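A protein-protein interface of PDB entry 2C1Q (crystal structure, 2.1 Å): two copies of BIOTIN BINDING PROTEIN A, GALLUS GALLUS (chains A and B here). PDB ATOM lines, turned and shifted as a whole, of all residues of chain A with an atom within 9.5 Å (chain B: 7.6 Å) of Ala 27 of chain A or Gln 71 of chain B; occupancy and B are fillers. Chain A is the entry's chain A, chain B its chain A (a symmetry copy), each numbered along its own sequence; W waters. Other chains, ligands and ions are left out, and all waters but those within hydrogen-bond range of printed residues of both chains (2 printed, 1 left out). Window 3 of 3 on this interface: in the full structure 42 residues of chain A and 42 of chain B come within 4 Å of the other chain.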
ATOM      1  N   ALA A  23     -11.384 -27.973  -8.866  1.00  0.00           N
ATOM      2  CA  ALA A  23     -10.067 -27.484  -8.408  1.00  0.00           C
ATOM      3  C   ALA A  23     -10.181 -26.585  -7.167  1.00  0.00           C
ATOM      4  O   ALA A  23     -11.114 -25.799  -7.019  1.00  0.00           O
ATOM      5  CB  ALA A  23      -9.316 -26.743  -9.541  1.00  0.00           C
ATOM      6  N   LEU A  24      -9.214 -26.728  -6.282  1.00  0.00           N
ATOM      7  CA  LEU A  24      -9.075 -25.845  -5.158  1.00  0.00           C
ATOM      8  C   LEU A  24      -8.488 -24.520  -5.606  1.00  0.00           C
ATOM      9  O   LEU A  24      -7.588 -24.484  -6.457  1.00  0.00           O
ATOM     10  CB  LEU A  24      -8.176 -26.493  -4.093  1.00  0.00           C
ATOM     11  CG  LEU A  24      -8.879 -27.477  -3.134  1.00  0.00           C
ATOM     12  CD1 LEU A  24      -9.546 -28.655  -3.865  1.00  0.00           C
ATOM     13  CD2 LEU A  24      -7.899 -27.972  -2.107  1.00  0.00           C
ATOM     14  N   ASP A  25      -9.002 -23.426  -5.042  1.00  0.00           N
ATOM     15  CA  ASP A  25      -8.306 -22.155  -5.168  1.00  0.00           C
ATOM     16  C   ASP A  25      -7.102 -22.137  -4.211  1.00  0.00           C
ATOM     17  O   ASP A  25      -6.885 -23.111  -3.485  1.00  0.00           O
ATOM     18  CB  ASP A  25      -9.273 -20.975  -5.013  1.00  0.00           C
ATOM     19  CG  ASP A  25      -9.734 -20.756  -3.593  1.00  0.00           C
ATOM     20  OD1 ASP A  25      -9.127 -21.305  -2.652  1.00  0.00           O
ATOM     21  OD2 ASP A  25     -10.728 -20.008  -3.422  1.00  0.00           O
ATOM     22  N   VAL A  26      -6.321 -21.050  -4.203  1.00  0.00           N
ATOM     23  CA  VAL A  26      -5.041 -21.019  -3.452  1.00  0.00           C
ATOM     24  C   VAL A  26      -5.270 -20.833  -1.939  1.00  0.00           C
ATOM     25  O   VAL A  26      -4.468 -21.281  -1.112  1.00  0.00           O
ATOM     26  CB  VAL A  26      -3.982 -20.022  -4.100  1.00  0.00           C
ATOM     27  CG1 VAL A  26      -4.641 -19.069  -5.107  1.00  0.00           C
ATOM     28  CG2 VAL A  26      -3.161 -19.252  -3.058  1.00  0.00           C
ATOM     29  N   ALA A  27      -6.389 -20.202  -1.590  1.00  0.00           N
ATOM     30  CA  ALA A  27      -6.891 -20.198  -0.217  1.00  0.00           C
ATOM     31  C   ALA A  27      -7.296 -21.603   0.316  1.00  0.00           C
ATOM     32  O   ALA A  27      -7.441 -21.790   1.524  1.00  0.00           O
ATOM     33  CB  ALA A  27      -8.042 -19.219  -0.084  1.00  0.00           C
ATOM     34  N   GLY A  28      -7.462 -22.580  -0.582  1.00  0.00           N
ATOM     35  CA  GLY A  28      -7.738 -23.955  -0.181  1.00  0.00           C
ATOM     36  C   GLY A  28      -9.225 -24.243  -0.177  1.00  0.00           C
ATOM     37  O   GLY A  28      -9.660 -25.344   0.200  1.00  0.00           O
ATOM     38  N   THR A  29     -10.014 -23.260  -0.597  1.00  0.00           N
ATOM     39  CA  THR A  29     -11.440 -23.473  -0.659  1.00  0.00           C
ATOM     40  C   THR A  29     -11.762 -24.196  -1.970  1.00  0.00           C
ATOM     41  O   THR A  29     -11.093 -24.016  -2.988  1.00  0.00           O
ATOM     42  CB  THR A  29     -12.242 -22.167  -0.500  1.00  0.00           C
ATOM     43  OG1 THR A  29     -11.865 -21.279  -1.529  1.00  0.00           O
ATOM     44  CG2 THR A  29     -11.927 -21.472   0.834  1.00  0.00           C
ATOM     45  N   PHE A  30     -12.779 -25.031  -1.939  1.00  0.00           N
ATOM     46  CA  PHE A  30     -13.205 -25.728  -3.138  1.00  0.00           C
ATOM     47  C   PHE A  30     -14.702 -25.803  -3.200  1.00  0.00           C
ATOM     48  O   PHE A  30     -15.386 -25.591  -2.206  1.00  0.00           O
ATOM     49  CB  PHE A  30     -12.603 -27.136  -3.183  1.00  0.00           C
ATOM     50  CG  PHE A  30     -12.893 -27.980  -1.958  1.00  0.00           C
ATOM     51  CD1 PHE A  30     -14.033 -28.757  -1.879  1.00  0.00           C
ATOM     52  CD2 PHE A  30     -11.995 -28.026  -0.906  1.00  0.00           C
ATOM     53  CE1 PHE A  30     -14.284 -29.561  -0.750  1.00  0.00           C
ATOM     54  CE2 PHE A  30     -12.245 -28.809   0.208  1.00  0.00           C
ATOM     55  CZ  PHE A  30     -13.391 -29.574   0.286  1.00  0.00           C
ATOM     56  N   LYS A  51     -19.625 -26.859  -0.840  1.00  0.00           N
ATOM     57  CA  LYS A  51     -18.681 -25.787  -0.572  1.00  0.00           C
ATOM     58  C   LYS A  51     -17.812 -26.210   0.610  1.00  0.00           C
ATOM     59  O   LYS A  51     -18.331 -26.494   1.698  1.00  0.00           O
ATOM     60  CB  LYS A  51     -19.460 -24.533  -0.163  1.00  0.00           C
ATOM     61  CG  LYS A  51     -18.631 -23.292  -0.019  1.00  0.00           C
ATOM     62  CD  LYS A  51     -17.931 -22.982  -1.340  1.00  0.00           C
ATOM     63  CE  LYS A  51     -17.998 -21.505  -1.671  1.00  0.00           C
ATOM     64  NZ  LYS A  51     -16.828 -21.096  -2.521  1.00  0.00           N
ATOM     65  N   GLY A  52     -16.505 -26.228   0.416  1.00  0.00           N
ATOM     66  CA  GLY A  52     -15.606 -26.634   1.476  1.00  0.00           C
ATOM     67  C   GLY A  52     -14.287 -25.933   1.454  1.00  0.00           C
ATOM     68  O   GLY A  52     -14.038 -25.086   0.599  1.00  0.00           O
ATOM     69  N   ALA A  53     -13.426 -26.316   2.390  1.00  0.00           N
ATOM     70  CA  ALA A  53     -12.064 -25.801   2.459  1.00  0.00           C
ATOM     71  C   ALA A  53     -11.183 -26.912   2.943  1.00  0.00           C
ATOM     72  O   ALA A  53     -11.603 -27.709   3.785  1.00  0.00           O
ATOM     73  CB  ALA A  53     -11.945 -24.603   3.422  1.00  0.00           C
ATOM     74  N   GLN A  54      -9.957 -26.945   2.420  1.00  0.00           N
ATOM     75  CA  GLN A  54      -8.918 -27.817   2.908  1.00  0.00           C
ATOM     76  C   GLN A  54      -7.808 -27.033   3.614  1.00  0.00           C
ATOM     77  O   GLN A  54      -7.517 -25.886   3.286  1.00  0.00           O
ATOM     78  CB  GLN A  54      -8.305 -28.577   1.754  1.00  0.00           C
ATOM     79  CG  GLN A  54      -7.301 -29.597   2.210  1.00  0.00           C
ATOM     80  CD  GLN A  54      -6.845 -30.516   1.098  1.00  0.00           C
ATOM     81  OE1 GLN A  54      -6.711 -30.106  -0.058  1.00  0.00           O
ATOM     82  NE2 GLN A  54      -6.600 -31.765   1.447  1.00  0.00           N
ATOM     83  N   GLN A  55      -7.158 -27.688   4.558  1.00  0.00           N
ATOM     84  CA  GLN A  55      -5.982 -27.132   5.221  1.00  0.00           C
ATOM     85  C   GLN A  55      -4.759 -27.149   4.288  1.00  0.00           C
ATOM     86  O   GLN A  55      -4.711 -27.951   3.367  1.00  0.00           O
ATOM     87  CB  GLN A  55      -5.715 -27.946   6.480  1.00  0.00           C
ATOM     88  CG  GLN A  55      -6.694 -27.661   7.599  1.00  0.00           C
ATOM     89  CD  GLN A  55      -6.334 -26.372   8.310  1.00  0.00           C
ATOM     90  OE1 GLN A  55      -5.486 -25.606   7.831  1.00  0.00           O
ATOM     91  NE2 GLN A  55      -6.949 -26.125   9.446  1.00  0.00           N
ATOM     92  N   PRO A  56      -3.786 -26.227   4.484  1.00  0.00           N
ATOM     93  CA  PRO A  56      -2.601 -26.300   3.617  1.00  0.00           C
ATOM     94  C   PRO A  56      -1.712 -27.526   3.870  1.00  0.00           C
ATOM     95  O   PRO A  56      -1.524 -27.926   5.032  1.00  0.00           O
ATOM     96  CB  PRO A  56      -1.842 -25.011   3.944  1.00  0.00           C
ATOM     97  CG  PRO A  56      -2.293 -24.636   5.319  1.00  0.00           C
ATOM     98  CD  PRO A  56      -3.731 -25.062   5.391  1.00  0.00           C
ATOM     99  N   PRO A  57      -1.184 -28.134   2.784  1.00  0.00           N
ATOM    100  CA  PRO A  57      -0.206 -29.226   2.928  1.00  0.00           C
ATOM    101  C   PRO A  57       1.169 -28.688   3.329  1.00  0.00           C
ATOM    102  O   PRO A  57       1.371 -28.320   4.495  1.00  0.00           O
ATOM    103  CB  PRO A  57      -0.169 -29.864   1.529  1.00  0.00           C
ATOM    104  CG  PRO A  57      -0.543 -28.753   0.596  1.00  0.00           C
ATOM    105  CD  PRO A  57      -1.495 -27.846   1.368  1.00  0.00           C
ATOM    106  N   PRO A  64      -3.534 -33.013   4.374  1.00  0.00           N
ATOM    107  CA  PRO A  64      -4.256 -32.106   5.258  1.00  0.00           C
ATOM    108  C   PRO A  64      -5.752 -32.461   5.428  1.00  0.00           C
ATOM    109  O   PRO A  64      -6.356 -33.080   4.540  1.00  0.00           O
ATOM    110  CB  PRO A  64      -4.088 -30.752   4.578  1.00  0.00           C
ATOM    111  CG  PRO A  64      -3.785 -31.047   3.177  1.00  0.00           C
ATOM    112  CD  PRO A  64      -3.200 -32.400   3.081  1.00  0.00           C
ATOM    113  N   THR A  65      -6.313 -32.100   6.582  1.00  0.00           N
ATOM    114  CA  THR A  65      -7.741 -32.319   6.851  1.00  0.00           C
ATOM    115  C   THR A  65      -8.564 -31.383   5.979  1.00  0.00           C
ATOM    116  O   THR A  65      -8.086 -30.312   5.590  1.00  0.00           O
ATOM    117  CB  THR A  65      -8.092 -32.100   8.335  1.00  0.00           C
ATOM    118  OG1 THR A  65      -7.733 -30.765   8.737  1.00  0.00           O
ATOM    119  CG2 THR A  65      -7.383 -33.125   9.239  1.00  0.00           C
ATOM    120  N   PHE A  66      -9.780 -31.790   5.623  1.00  0.00           N
ATOM    121  CA  PHE A  66     -10.695 -30.878   4.939  1.00  0.00           C
ATOM    122  C   PHE A  66     -12.119 -31.044   5.437  1.00  0.00           C
ATOM    123  O   PHE A  66     -12.424 -31.969   6.162  1.00  0.00           O
ATOM    124  CB  PHE A  66     -10.647 -31.130   3.427  1.00  0.00           C
ATOM    125  CG  PHE A  66     -10.989 -32.527   3.058  1.00  0.00           C
ATOM    126  CD1 PHE A  66     -12.270 -32.854   2.635  1.00  0.00           C
ATOM    127  CD2 PHE A  66     -10.051 -33.553   3.194  1.00  0.00           C
ATOM    128  CE1 PHE A  66     -12.581 -34.193   2.300  1.00  0.00           C
ATOM    129  CE2 PHE A  66     -10.369 -34.879   2.868  1.00  0.00           C
ATOM    130  CZ  PHE A  66     -11.640 -35.191   2.428  1.00  0.00           C
ATOM    131  N   GLY A  67     -12.998 -30.138   5.040  1.00  0.00           N
ATOM    132  CA  GLY A  67     -14.420 -30.257   5.361  1.00  0.00           C
ATOM    133  C   GLY A  67     -15.233 -29.637   4.275  1.00  0.00           C
ATOM    134  O   GLY A  67     -14.738 -28.800   3.556  1.00  0.00           O
ATOM    135  N   VAL A  82     -16.349 -34.107   7.233  1.00  0.00           N
ATOM    136  CA  VAL A  82     -15.004 -33.723   7.599  1.00  0.00           C
ATOM    137  C   VAL A  82     -14.087 -34.974   7.447  1.00  0.00           C
ATOM    138  O   VAL A  82     -14.515 -36.119   7.715  1.00  0.00           O
ATOM    139  CB  VAL A  82     -15.013 -33.026   8.993  1.00  0.00           C
ATOM    140  CG1 VAL A  82     -15.326 -34.023  10.133  1.00  0.00           C
ATOM    141  CG2 VAL A  82     -13.726 -32.241   9.251  1.00  0.00           C
ATOM    142  N   TYR B  34     -13.892 -17.161  12.660  1.00  0.00           N
ATOM    143  CA  TYR B  34     -14.210 -17.794  13.905  1.00  0.00           C
ATOM    144  C   TYR B  34     -13.057 -17.565  14.850  1.00  0.00           C
ATOM    145  O   TYR B  34     -11.908 -17.888  14.529  1.00  0.00           O
ATOM    146  CB  TYR B  34     -14.360 -19.309  13.687  1.00  0.00           C
ATOM    147  CG  TYR B  34     -15.222 -19.993  14.706  1.00  0.00           C
ATOM    148  CD1 TYR B  34     -16.588 -20.196  14.464  1.00  0.00           C
ATOM    149  CD2 TYR B  34     -14.690 -20.450  15.910  1.00  0.00           C
ATOM    150  CE1 TYR B  34     -17.398 -20.838  15.422  1.00  0.00           C
ATOM    151  CE2 TYR B  34     -15.492 -21.091  16.860  1.00  0.00           C
ATOM    152  CZ  TYR B  34     -16.828 -21.263  16.615  1.00  0.00           C
ATOM    153  OH  TYR B  34     -17.596 -21.884  17.551  1.00  0.00           O
ATOM    154  N   LEU B  46      -5.602 -18.479  16.925  1.00  0.00           N
ATOM    155  CA  LEU B  46      -5.664 -17.395  15.936  1.00  0.00           C
ATOM    156  C   LEU B  46      -7.014 -17.397  15.244  1.00  0.00           C
ATOM    157  O   LEU B  46      -7.544 -18.493  14.961  1.00  0.00           O
ATOM    158  CB  LEU B  46      -4.604 -17.601  14.847  1.00  0.00           C
ATOM    159  CG  LEU B  46      -3.112 -17.524  15.198  1.00  0.00           C
ATOM    160  CD1 LEU B  46      -2.352 -17.132  13.947  1.00  0.00           C
ATOM    161  CD2 LEU B  46      -2.813 -16.500  16.320  1.00  0.00           C
ATOM    162  N   VAL B  47      -7.567 -16.200  14.975  1.00  0.00           N
ATOM    163  CA  VAL B  47      -8.770 -16.063  14.138  1.00  0.00           C
ATOM    164  C   VAL B  47      -8.587 -16.860  12.831  1.00  0.00           C
ATOM    165  O   VAL B  47      -7.489 -16.894  12.242  1.00  0.00           O
ATOM    166  CB  VAL B  47      -9.133 -14.572  13.812  1.00  0.00           C
ATOM    167  CG1 VAL B  47      -7.960 -13.829  13.099  1.00  0.00           C
ATOM    168  CG2 VAL B  47     -10.411 -14.494  12.994  1.00  0.00           C
ATOM    169  N   SER B  48      -9.664 -17.521  12.418  1.00  0.00           N
ATOM    170  CA  SER B  48      -9.627 -18.499  11.345  1.00  0.00           C
ATOM    171  C   SER B  48     -10.766 -18.298  10.378  1.00  0.00           C
ATOM    172  O   SER B  48     -11.882 -18.016  10.808  1.00  0.00           O
ATOM    173  CB  SER B  48      -9.691 -19.897  11.942  1.00  0.00           C
ATOM    174  OG  SER B  48      -8.461 -20.210  12.559  1.00  0.00           O
ATOM    175  N   PRO B  49     -10.496 -18.441   9.061  1.00  0.00           N
ATOM    176  CA  PRO B  49     -11.553 -18.254   8.083  1.00  0.00           C
ATOM    177  C   PRO B  49     -12.588 -19.376   8.174  1.00  0.00           C
ATOM    178  O   PRO B  49     -12.237 -20.487   8.534  1.00  0.00           O
ATOM    179  CB  PRO B  49     -10.805 -18.323   6.740  1.00  0.00           C
ATOM    180  CG  PRO B  49      -9.599 -19.089   7.021  1.00  0.00           C
ATOM    181  CD  PRO B  49      -9.216 -18.825   8.427  1.00  0.00           C
ATOM    182  N   LEU B  50     -13.853 -19.082   7.880  1.00  0.00           N
ATOM    183  CA  LEU B  50     -14.833 -20.129   7.642  1.00  0.00           C
ATOM    184  C   LEU B  50     -15.529 -19.938   6.282  1.00  0.00           C
ATOM    185  O   LEU B  50     -15.615 -18.824   5.750  1.00  0.00           O
ATOM    186  CB  LEU B  50     -15.878 -20.206   8.783  1.00  0.00           C
ATOM    187  CG  LEU B  50     -16.871 -19.035   8.929  1.00  0.00           C
ATOM    188  CD1 LEU B  50     -18.095 -19.168   8.052  1.00  0.00           C
ATOM    189  CD2 LEU B  50     -17.278 -18.861  10.371  1.00  0.00           C
ATOM    190  N   LYS B  51     -16.045 -21.051   5.761  1.00  0.00           N
ATOM    191  CA  LYS B  51     -16.735 -21.133   4.484  1.00  0.00           C
ATOM    192  C   LYS B  51     -17.947 -22.044   4.662  1.00  0.00           C
ATOM    193  O   LYS B  51     -17.801 -23.211   5.052  1.00  0.00           O
ATOM    194  CB  LYS B  51     -15.799 -21.783   3.458  1.00  0.00           C
ATOM    195  CG  LYS B  51     -16.309 -21.782   2.048  1.00  0.00           C
ATOM    196  CD  LYS B  51     -16.560 -20.347   1.590  1.00  0.00           C
ATOM    197  CE  LYS B  51     -16.053 -20.117   0.182  1.00  0.00           C
ATOM    198  NZ  LYS B  51     -16.837 -19.028  -0.496  1.00  0.00           N
ATOM    199  N   PHE B  68     -21.004 -24.936   8.013  1.00  0.00           N
ATOM    200  CA  PHE B  68     -19.740 -24.376   7.547  1.00  0.00           C
ATOM    201  C   PHE B  68     -18.533 -25.152   8.016  1.00  0.00           C
ATOM    202  O   PHE B  68     -18.617 -25.947   8.942  1.00  0.00           O
ATOM    203  CB  PHE B  68     -19.605 -22.912   7.964  1.00  0.00           C
ATOM    204  CG  PHE B  68     -19.713 -22.671   9.454  1.00  0.00           C
ATOM    205  CD1 PHE B  68     -18.581 -22.665  10.244  1.00  0.00           C
ATOM    206  CD2 PHE B  68     -20.945 -22.391  10.049  1.00  0.00           C
ATOM    207  CE1 PHE B  68     -18.642 -22.433  11.597  1.00  0.00           C
ATOM    208  CE2 PHE B  68     -21.011 -22.124  11.431  1.00  0.00           C
ATOM    209  CZ  PHE B  68     -19.882 -22.163  12.199  1.00  0.00           C
ATOM    210  N   THR B  69     -17.401 -24.854   7.381  1.00  0.00           N
ATOM    211  CA  THR B  69     -16.121 -25.456   7.662  1.00  0.00           C
ATOM    212  C   THR B  69     -15.231 -24.336   8.198  1.00  0.00           C
ATOM    213  O   THR B  69     -15.208 -23.242   7.648  1.00  0.00           O
ATOM    214  CB  THR B  69     -15.510 -26.009   6.352  1.00  0.00           C
ATOM    215  OG1 THR B  69     -16.426 -26.941   5.748  1.00  0.00           O
ATOM    216  CG2 THR B  69     -14.199 -26.701   6.605  1.00  0.00           C
ATOM    217  N   VAL B  70     -14.547 -24.586   9.305  1.00  0.00           N
ATOM    218  CA  VAL B  70     -13.563 -23.649   9.811  1.00  0.00           C
ATOM    219  C   VAL B  70     -12.179 -24.232   9.494  1.00  0.00           C
ATOM    220  O   VAL B  70     -11.866 -25.372   9.850  1.00  0.00           O
ATOM    221  CB  VAL B  70     -13.663 -23.428  11.342  1.00  0.00           C
ATOM    222  CG1 VAL B  70     -12.615 -22.413  11.769  1.00  0.00           C
ATOM    223  CG2 VAL B  70     -15.086 -22.957  11.747  1.00  0.00           C
ATOM    224  N   GLN B  71     -11.375 -23.440   8.803  1.00  0.00           N
ATOM    225  CA  GLN B  71     -10.003 -23.792   8.493  1.00  0.00           C
ATOM    226  C   GLN B  71      -9.106 -23.211   9.553  1.00  0.00           C
ATOM    227  O   GLN B  71      -8.685 -22.067   9.422  1.00  0.00           O
ATOM    228  CB  GLN B  71      -9.675 -23.139   7.167  1.00  0.00           C
ATOM    229  CG  GLN B  71      -8.446 -23.613   6.481  1.00  0.00           C
ATOM    230  CD  GLN B  71      -8.158 -22.742   5.263  1.00  0.00           C
ATOM    231  OE1 GLN B  71      -7.911 -21.540   5.406  1.00  0.00           O
ATOM    232  NE2 GLN B  71      -8.186 -23.340   4.062  1.00  0.00           N
ATOM    233  N   TRP B  72      -8.807 -23.971  10.605  1.00  0.00           N
ATOM    234  CA  TRP B  72      -8.050 -23.401  11.731  1.00  0.00           C
ATOM    235  C   TRP B  72      -6.668 -22.927  11.314  1.00  0.00           C
ATOM    236  O   TRP B  72      -5.922 -23.670  10.682  1.00  0.00           O
ATOM    237  CB  TRP B  72      -7.950 -24.388  12.901  1.00  0.00           C
ATOM    238  CG  TRP B  72      -9.305 -24.811  13.386  1.00  0.00           C
ATOM    239  CD1 TRP B  72      -9.887 -26.036  13.212  1.00  0.00           C
ATOM    240  CD2 TRP B  72     -10.273 -23.997  14.058  1.00  0.00           C
ATOM    241  NE1 TRP B  72     -11.146 -26.045  13.747  1.00  0.00           N
ATOM    242  CE2 TRP B  72     -11.408 -24.811  14.289  1.00  0.00           C
ATOM    243  CE3 TRP B  72     -10.273 -22.672  14.544  1.00  0.00           C
ATOM    244  CZ2 TRP B  72     -12.542 -24.342  14.936  1.00  0.00           C
ATOM    245  CZ3 TRP B  72     -11.399 -22.205  15.195  1.00  0.00           C
ATOM    246  CH2 TRP B  72     -12.527 -23.053  15.398  1.00  0.00           C
ATOM    247  N   GLN B  73      -6.309 -21.695  11.695  1.00  0.00           N
ATOM    248  CA  GLN B  73      -5.024 -21.151  11.241  1.00  0.00           C
ATOM    249  C   GLN B  73      -3.813 -21.542  12.087  1.00  0.00           C
ATOM    250  O   GLN B  73      -2.668 -21.268  11.711  1.00  0.00           O
ATOM    251  CB  GLN B  73      -5.109 -19.636  11.026  1.00  0.00           C
ATOM    252  CG  GLN B  73      -5.941 -19.281   9.821  1.00  0.00           C
ATOM    253  CD  GLN B  73      -5.432 -19.898   8.531  1.00  0.00           C
ATOM    254  OE1 GLN B  73      -4.285 -19.670   8.133  1.00  0.00           O
ATOM    255  NE2 GLN B  73      -6.289 -20.677   7.859  1.00  0.00           N
ATOM    256  N   PHE B  74      -4.066 -22.231  13.199  1.00  0.00           N
ATOM    257  CA  PHE B  74      -3.014 -22.532  14.165  1.00  0.00           C
ATOM    258  C   PHE B  74      -2.976 -24.024  14.506  1.00  0.00           C
ATOM    259  O   PHE B  74      -2.284 -24.441  15.426  1.00  0.00           O
ATOM    260  CB  PHE B  74      -3.301 -21.747  15.431  1.00  0.00           C
ATOM    261  CG  PHE B  74      -4.651 -22.072  16.045  1.00  0.00           C
ATOM    262  CD1 PHE B  74      -4.777 -23.090  17.000  1.00  0.00           C
ATOM    263  CD2 PHE B  74      -5.799 -21.379  15.649  1.00  0.00           C
ATOM    264  CE1 PHE B  74      -6.040 -23.403  17.562  1.00  0.00           C
ATOM    265  CE2 PHE B  74      -7.040 -21.680  16.209  1.00  0.00           C
ATOM    266  CZ  PHE B  74      -7.151 -22.698  17.165  1.00  0.00           C
ATOM    267  N   ALA B  75      -3.765 -24.822  13.791  1.00  0.00           N
ATOM    268  CA  ALA B  75      -3.896 -26.232  14.108  1.00  0.00           C
ATOM    269  C   ALA B  75      -4.037 -27.024  12.826  1.00  0.00           C
ATOM    270  O   ALA B  75      -4.568 -26.516  11.844  1.00  0.00           O
ATOM    271  CB  ALA B  75      -5.106 -26.455  15.008  1.00  0.00           C
ATOM    272  N   SER B  77      -6.076 -29.265  12.338  1.00  0.00           N
ATOM    273  CA  SER B  77      -7.421 -29.807  12.320  1.00  0.00           C
ATOM    274  C   SER B  77      -8.417 -29.034  11.444  1.00  0.00           C
ATOM    275  O   SER B  77      -8.081 -27.999  10.864  1.00  0.00           O
ATOM    276  CB  SER B  77      -7.897 -29.829  13.751  1.00  0.00           C
ATOM    277  OG  SER B  77      -7.922 -28.501  14.213  1.00  0.00           O
ATOM    278  N   THR B  78      -9.641 -29.557  11.351  1.00  0.00           N
ATOM    279  CA  THR B  78     -10.722 -28.911  10.644  1.00  0.00           C
ATOM    280  C   THR B  78     -12.011 -29.185  11.417  1.00  0.00           C
ATOM    281  O   THR B  78     -12.242 -30.306  11.839  1.00  0.00           O
ATOM    282  CB  THR B  78     -10.849 -29.438   9.195  1.00  0.00           C
ATOM    283  OG1 THR B  78      -9.635 -29.156   8.475  1.00  0.00           O
ATOM    284  CG2 THR B  78     -11.932 -28.756   8.501  1.00  0.00           C
ATOM    285  N   THR B  79     -12.807 -28.152  11.661  1.00  0.00           N
ATOM    286  CA  THR B  79     -14.126 -28.345  12.258  1.00  0.00           C
ATOM    287  C   THR B  79     -15.203 -28.028  11.261  1.00  0.00           C
ATOM    288  O   THR B  79     -15.082 -27.066  10.492  1.00  0.00           O
ATOM    289  CB  THR B  79     -14.374 -27.471  13.509  1.00  0.00           C
ATOM    290  OG1 THR B  79     -13.383 -27.750  14.489  1.00  0.00           O
ATOM    291  CG2 THR B  79     -15.746 -27.825  14.137  1.00  0.00           C
HETATM  292  O   HOH W   1      -9.993 -26.866   6.416  1.00  0.00           O
HETATM  293  O   HOH W   2     -18.282 -25.690   4.229  1.00  0.00           O
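NE2 of Gln 55 of chain A sits at hydrogen-bond distance from O of Ser 77 of chain B, 2.6 Å away.
The backbone carbonyl oxygen (O) of Trp 72 of chain B sits at hydrogen-bond distance from the side-chain amide nitrogen (NE2) of Gln 55 of chain A (2.9 Å).
The side-chain hydroxyl of Thr 65 of chain A sits at hydrogen-bond distance from the side-chain hydroxyl of Thr 78 of chain B, at 2.5 Å.
The backbone carbonyl oxygen of Gly 67 of chain A lies close to the side-chain hydroxyl of Thr 69 of chain B (3.3 Å).
The backbone carbonyl oxygen (O) of Gln 54 of chain A is in hydrogen-bond range of the side-chain amide nitrogen (NE2) of Gln 71 of chain B, at 2.7 Å.
NZ of Lys 51 of chain A sits close to NZ of Lys 51 of chain B (2.9 Å).
The backbone carbonyl oxygen (O) of Ala 27 of chain A lies within hydrogen-bond range of the side-chain amide nitrogen (NE2) of Gln 71 of chain B.
NE2 of Gln 55 of chain A is in hydrogen-bond range of O of Ala 75 of chain B, at 3.4 Å.
Hydrophobic or aromatic side chains of chain A that line the printed part of chain B: Val 82.
Hydrophobic or aromatic side chains of chain B within 4 Å of the printed part of chain A: Trp 72.
Ala 27 of chain A touches one residue of chain B.
Of the printed residues of chain B, Gln 55 of chain A touches Gln 71 (3.6 Å), Trp 72 (2.9 Å), Ala 75 (3.4 Å), Ser 77 (2.6 Å) and Thr 78 (3.4 Å).
Of the printed residues of chain B, Gly 67 of chain A touches Thr 69 (3.3 Å) and Thr 78 (3.9 Å).
Of the printed residues of chain B, Val 82 of chain A touches Thr 78 (3.6 Å).
Leu 46 of chain B touches none of the printed residues of chain A.
No residue of chain A comes within 4 Å of Pro 49 of chain B.
Phe 68 of chain B touches none of the printed residues of chain A.
Printed residues of chain A within 4 Å of Thr 69 of chain B: Ala 53 and Gly 67.
Of the printed residues of chain A, Gln 71 of chain B touches Ala 27 (3.1 Å), Gln 54 (2.7 Å) and Gln 55 (3.6 Å).
Of the printed residues of chain A, Thr 78 of chain B touches Gln 55 (3.4 Å), Thr 65 (2.5 Å), Phe 66 (3.8 Å), Gly 67 (3.9 Å) and Val 82 (3.6 Å).
The nearest residue of chain B that does not touch Ala 27 of chain A is Pro 49 of chain B (6.5 Å).
The nearest printed residue of chain A that does not touch Gln 71 of chain B is Ala 53 of chain A (4.02 Å).
Lys 51 of chain B touches its own counterpart, Lys 51 of chain A.
Position printed for both chains: 51.
Among the printed residues, pairs that only touch across the chains: Ala 53 of chain A with Thr 69 of chain B (3.96 Å), Gln 55 of chain A with Gln 71 of chain B (3.6 Å), Gln 55 of chain A with Thr 78 of chain B (3.4 Å), Thr 65 of chain A with Ser 77 of chain B (3.3 Å), Phe 66 of chain A with Thr 78 of chain B (3.8 Å), Gly 67 of chain A with Thr 78 of chain B (3.9 Å) and Val 82 of chain A with Thr 78 of chain B (3.6 Å).
Water W2 lies within hydrogen-bond range of O of Lys 51 of chain A (2.7 Å), O of Lys 51 of chain B (2.7 Å) and OG1 of Thr 69 of chain B (2.7 Å).
Water W1 lies within hydrogen-bond range of OG1 of Thr 78 of chain B (3.1 Å), O of Ala 53 of chain A (3.2 Å) and N of Gln 55 of chain A (3.5 Å).
The backbone NH of Ala 27 of chain A sits at hydrogen-bond distance from the side-chain carboxylate of Asp 25 of chain A, at 3.1 Å.
O of Thr 65 of chain A sits at hydrogen-bond distance from N of Gln 55 of chain A.
The backbone NH (N) of Ala 53 of chain A lies within hydrogen-bond range of the backbone carbonyl oxygen (O) of Gly 67 of chain A (3.0 Å).
OE1 of Gln 71 of chain B sits at hydrogen-bond distance from NE2 of Gln 73 of chain B (3.1 Å).
N of Gln 71 of chain B is in hydrogen-bond range of O of Pro 49 of chain B (3.1 Å).
NE1 of Trp 72 of chain B sits at hydrogen-bond distance from OG1 of Thr 79 of chain B, at 2.9 Å.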
